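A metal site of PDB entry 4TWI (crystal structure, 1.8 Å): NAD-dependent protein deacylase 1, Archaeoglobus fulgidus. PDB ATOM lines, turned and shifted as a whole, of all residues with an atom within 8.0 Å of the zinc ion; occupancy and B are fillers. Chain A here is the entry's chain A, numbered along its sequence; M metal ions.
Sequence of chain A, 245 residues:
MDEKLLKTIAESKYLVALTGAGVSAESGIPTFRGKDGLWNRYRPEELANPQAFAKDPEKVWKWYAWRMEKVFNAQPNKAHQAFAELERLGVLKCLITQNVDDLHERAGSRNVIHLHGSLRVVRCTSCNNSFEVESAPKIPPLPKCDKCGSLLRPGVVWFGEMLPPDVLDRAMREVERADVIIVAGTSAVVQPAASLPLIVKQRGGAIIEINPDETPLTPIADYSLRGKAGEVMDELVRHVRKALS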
ATOM      1  N   ARG A 123      -7.263   1.986 -27.747  1.00  0.00           N
ATOM      2  CA  ARG A 123      -6.738   2.804 -26.667  1.00  0.00           C
ATOM      3  C   ARG A 123      -7.127   4.268 -26.791  1.00  0.00           C
ATOM      4  O   ARG A 123      -7.504   4.737 -27.863  1.00  0.00           O
ATOM      5  CB  ARG A 123      -5.223   2.659 -26.559  1.00  0.00           C
ATOM      6  CG  ARG A 123      -4.426   3.223 -27.718  1.00  0.00           C
ATOM      7  CD  ARG A 123      -2.969   3.365 -27.283  1.00  0.00           C
ATOM      8  NE  ARG A 123      -2.093   3.823 -28.357  1.00  0.00           N
ATOM      9  CZ  ARG A 123      -1.794   5.101 -28.630  1.00  0.00           C
ATOM     10  NH1 ARG A 123      -2.313   6.112 -27.925  1.00  0.00           N
ATOM     11  NH2 ARG A 123      -0.962   5.358 -29.624  1.00  0.00           N
ATOM     12  N   CYS A 124      -7.031   4.968 -25.677  1.00  0.00           N
ATOM     13  CA  CYS A 124      -7.339   6.383 -25.647  1.00  0.00           C
ATOM     14  C   CYS A 124      -6.213   7.202 -26.260  1.00  0.00           C
ATOM     15  O   CYS A 124      -5.031   6.866 -26.113  1.00  0.00           O
ATOM     16  CB  CYS A 124      -7.605   6.838 -24.224  1.00  0.00           C
ATOM     17  SG  CYS A 124      -8.329   8.476 -24.169  1.00  0.00           S
ATOM     18  N   THR A 125      -6.584   8.285 -26.939  1.00  0.00           N
ATOM     19  CA  THR A 125      -5.611   9.228 -27.488  1.00  0.00           C
ATOM     20  C   THR A 125      -5.019  10.150 -26.420  1.00  0.00           C
ATOM     21  O   THR A 125      -4.007  10.800 -26.659  1.00  0.00           O
ATOM     22  CB  THR A 125      -6.229  10.106 -28.584  1.00  0.00           C
ATOM     23  OG1 THR A 125      -7.412  10.742 -28.102  1.00  0.00           O
ATOM     24  CG2 THR A 125      -6.557   9.272 -29.823  1.00  0.00           C
ATOM     25  N   SER A 126      -5.652  10.219 -25.249  1.00  0.00           N
ATOM     26  CA  SER A 126      -5.252  11.150 -24.195  1.00  0.00           C
ATOM     27  C   SER A 126      -4.776  10.472 -22.913  1.00  0.00           C
ATOM     28  O   SER A 126      -3.602  10.609 -22.524  1.00  0.00           O
ATOM     29  CB  SER A 126      -6.413  12.105 -23.884  1.00  0.00           C
ATOM     30  OG  SER A 126      -6.021  13.087 -22.959  1.00  0.00           O
ATOM     31  N   CYS A 127      -5.669   9.745 -22.243  1.00  0.00           N
ATOM     32  CA  CYS A 127      -5.320   9.051 -20.997  1.00  0.00           C
ATOM     33  C   CYS A 127      -4.687   7.693 -21.309  1.00  0.00           C
ATOM     34  O   CYS A 127      -4.434   7.361 -22.462  1.00  0.00           O
ATOM     35  CB  CYS A 127      -6.555   8.929 -20.075  1.00  0.00           C
ATOM     36  SG  CYS A 127      -7.745   7.628 -20.437  1.00  0.00           S
ATOM     37  N   ASN A 128      -4.407   6.910 -20.260  1.00  0.00           N
ATOM     38  CA  ASN A 128      -3.719   5.628 -20.433  1.00  0.00           C
ATOM     39  C   ASN A 128      -4.661   4.452 -20.621  1.00  0.00           C
ATOM     40  O   ASN A 128      -4.221   3.295 -20.613  1.00  0.00           O
ATOM     41  CB  ASN A 128      -2.777   5.386 -19.250  1.00  0.00           C
ATOM     42  CG  ASN A 128      -1.595   6.338 -19.232  1.00  0.00           C
ATOM     43  OD1 ASN A 128      -1.101   6.756 -20.291  1.00  0.00           O
ATOM     44  ND2 ASN A 128      -1.127   6.685 -18.041  1.00  0.00           N
ATOM     45  N   ASN A 129      -5.947   4.733 -20.812  1.00  0.00           N
ATOM     46  CA  ASN A 129      -6.943   3.687 -20.967  1.00  0.00           C
ATOM     47  C   ASN A 129      -6.690   2.848 -22.206  1.00  0.00           C
ATOM     48  O   ASN A 129      -6.446   3.383 -23.286  1.00  0.00           O
ATOM     49  CB  ASN A 129      -8.351   4.274 -21.047  1.00  0.00           C
ATOM     50  CG  ASN A 129      -9.437   3.213 -21.071  1.00  0.00           C
ATOM     51  OD1 ASN A 129      -9.276   2.128 -20.494  1.00  0.00           O
ATOM     52  ND2 ASN A 129     -10.535   3.501 -21.748  1.00  0.00           N
ATOM     53  N   SER A 130      -6.759   1.534 -22.049  1.00  0.00           N
ATOM     54  CA  SER A 130      -6.468   0.595 -23.132  1.00  0.00           C
ATOM     55  C   SER A 130      -7.201  -0.707 -22.839  1.00  0.00           C
ATOM     56  O   SER A 130      -7.300  -1.108 -21.682  1.00  0.00           O
ATOM     57  CB  SER A 130      -4.962   0.344 -23.215  1.00  0.00           C
ATOM     58  OG  SER A 130      -4.633  -0.472 -24.308  1.00  0.00           O
ATOM     59  N   LYS A 144     -15.493   6.894 -28.231  1.00  0.00           N
ATOM     60  CA  LYS A 144     -14.958   7.775 -27.192  1.00  0.00           C
ATOM     61  C   LYS A 144     -14.609   6.981 -25.938  1.00  0.00           C
ATOM     62  O   LYS A 144     -15.297   6.022 -25.599  1.00  0.00           O
ATOM     63  CB  LYS A 144     -15.965   8.863 -26.809  1.00  0.00           C
ATOM     64  CG  LYS A 144     -16.380   9.782 -27.949  1.00  0.00           C
ATOM     65  CD  LYS A 144     -15.185  10.454 -28.605  1.00  0.00           C
ATOM     66  CE  LYS A 144     -15.623  11.526 -29.581  1.00  0.00           C
ATOM     67  NZ  LYS A 144     -14.465  12.032 -30.378  1.00  0.00           N
ATOM     68  N   CYS A 145     -13.550   7.422 -25.264  1.00  0.00           N
ATOM     69  CA  CYS A 145     -13.060   6.800 -24.033  1.00  0.00           C
ATOM     70  C   CYS A 145     -14.089   6.881 -22.907  1.00  0.00           C
ATOM     71  O   CYS A 145     -14.597   7.955 -22.585  1.00  0.00           O
ATOM     72  CB  CYS A 145     -11.762   7.490 -23.600  1.00  0.00           C
ATOM     73  SG  CYS A 145     -10.964   6.804 -22.140  1.00  0.00           S
ATOM     74  N   ASP A 146     -14.390   5.725 -22.306  1.00  0.00           N
ATOM     75  CA  ASP A 146     -15.345   5.659 -21.194  1.00  0.00           C
ATOM     76  C   ASP A 146     -14.818   6.326 -19.926  1.00  0.00           C
ATOM     77  O   ASP A 146     -15.607   6.735 -19.059  1.00  0.00           O
ATOM     78  CB  ASP A 146     -15.705   4.198 -20.896  1.00  0.00           C
ATOM     79  N   LYS A 147     -13.492   6.454 -19.818  1.00  0.00           N
ATOM     80  CA  LYS A 147     -12.849   7.038 -18.630  1.00  0.00           C
ATOM     81  C   LYS A 147     -12.769   8.572 -18.685  1.00  0.00           C
ATOM     82  O   LYS A 147     -13.098   9.238 -17.695  1.00  0.00           O
ATOM     83  CB  LYS A 147     -11.452   6.446 -18.424  1.00  0.00           C
ATOM     84  CG  LYS A 147     -11.454   5.029 -17.899  1.00  0.00           C
ATOM     85  CD  LYS A 147     -10.041   4.535 -17.611  1.00  0.00           C
ATOM     86  CE  LYS A 147     -10.026   3.328 -16.686  1.00  0.00           C
ATOM     87  NZ  LYS A 147     -10.702   2.133 -17.277  1.00  0.00           N
ATOM     88  N   CYS A 148     -12.342   9.122 -19.817  1.00  0.00           N
ATOM     89  CA  CYS A 148     -12.126  10.577 -19.938  1.00  0.00           C
ATOM     90  C   CYS A 148     -12.938  11.272 -21.039  1.00  0.00           C
ATOM     91  O   CYS A 148     -12.973  12.508 -21.072  1.00  0.00           O
ATOM     92  CB  CYS A 148     -10.642  10.867 -20.147  1.00  0.00           C
ATOM     93  SG  CYS A 148     -10.052  10.562 -21.836  1.00  0.00           S
ATOM     94  N   GLY A 149     -13.558  10.518 -21.937  1.00  0.00           N
ATOM     95  CA  GLY A 149     -14.365  11.098 -23.019  1.00  0.00           C
ATOM     96  C   GLY A 149     -13.604  11.502 -24.277  1.00  0.00           C
ATOM     97  O   GLY A 149     -14.203  12.006 -25.238  1.00  0.00           O
ATOM     98  N   SER A 150     -12.290  11.282 -24.299  1.00  0.00           N
ATOM     99  CA  SER A 150     -11.474  11.620 -25.464  1.00  0.00           C
ATOM    100  C   SER A 150     -11.628  10.580 -26.567  1.00  0.00           C
ATOM    101  O   SER A 150     -12.134   9.470 -26.335  1.00  0.00           O
ATOM    102  CB  SER A 150     -10.003  11.761 -25.086  1.00  0.00           C
ATOM    103  OG  SER A 150      -9.800  12.844 -24.194  1.00  0.00           O
ATOM    104  N   LEU A 151     -11.199  10.943 -27.765  1.00  0.00           N
ATOM    105  CA  LEU A 151     -11.265  10.060 -28.920  1.00  0.00           C
ATOM    106  C   LEU A 151     -10.408   8.816 -28.688  1.00  0.00           C
ATOM    107  O   LEU A 151      -9.293   8.919 -28.189  1.00  0.00           O
ATOM    108  CB  LEU A 151     -10.768  10.829 -30.152  1.00  0.00           C
ATOM    109  CG  LEU A 151     -10.775  10.159 -31.524  1.00  0.00           C
ATOM    110  CD1 LEU A 151     -12.174   9.685 -31.930  1.00  0.00           C
ATOM    111  CD2 LEU A 151     -10.233  11.134 -32.552  1.00  0.00           C
ATOM    112  N   LEU A 152     -10.953   7.649 -29.016  1.00  0.00           N
ATOM    113  CA  LEU A 152     -10.179   6.397 -29.008  1.00  0.00           C
ATOM    114  C   LEU A 152      -9.536   6.190 -30.368  1.00  0.00           C
ATOM    115  O   LEU A 152      -9.921   6.818 -31.356  1.00  0.00           O
ATOM    116  CB  LEU A 152     -11.077   5.199 -28.686  1.00  0.00           C
ATOM    117  CG  LEU A 152     -11.658   5.117 -27.281  1.00  0.00           C
ATOM    118  CD1 LEU A 152     -12.805   4.116 -27.225  1.00  0.00           C
ATOM    119  CD2 LEU A 152     -10.587   4.775 -26.252  1.00  0.00           C
HETATM  120 ZN    ZN M   1      -9.261   8.362 -21.986  1.00  0.00          ZN
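The backbone NH of Cys 145 sits at hydrogen-bond distance from the backbone carbonyl oxygen of Ser 150 (2.7 Å).
The backbone NH (N) of Ser 126 sits close to the side-chain sulfur (SG) of Cys 124, 3.4 Å away.
The side-chain sulfur (SG) of Cys 145 lies close to the side-chain amide nitrogen (ND2) of Asn 129 (3.4 Å).
The side-chain sulfur (SG) of Cys 145 sits close to the backbone NH (N) of Lys 147 (3.5 Å).
SG of Cys 148 lies close to OG of Ser 150, at 3.3 Å.
N of Cys 124 is in hydrogen-bond range of O of Asn 129 (2.9 Å).
The backbone NH (N) of Asn 129 sits close to the side-chain sulfur (SG) of Cys 127 (3.4 Å).
The zinc ion is bound by SG of Cys 127 (2.3 Å), SG of Cys 145 (2.3 Å), SG of Cys 148 (2.3 Å) and SG of Cys 124 (2.4 Å).
The zinc ion has four donor atoms within binding distance.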
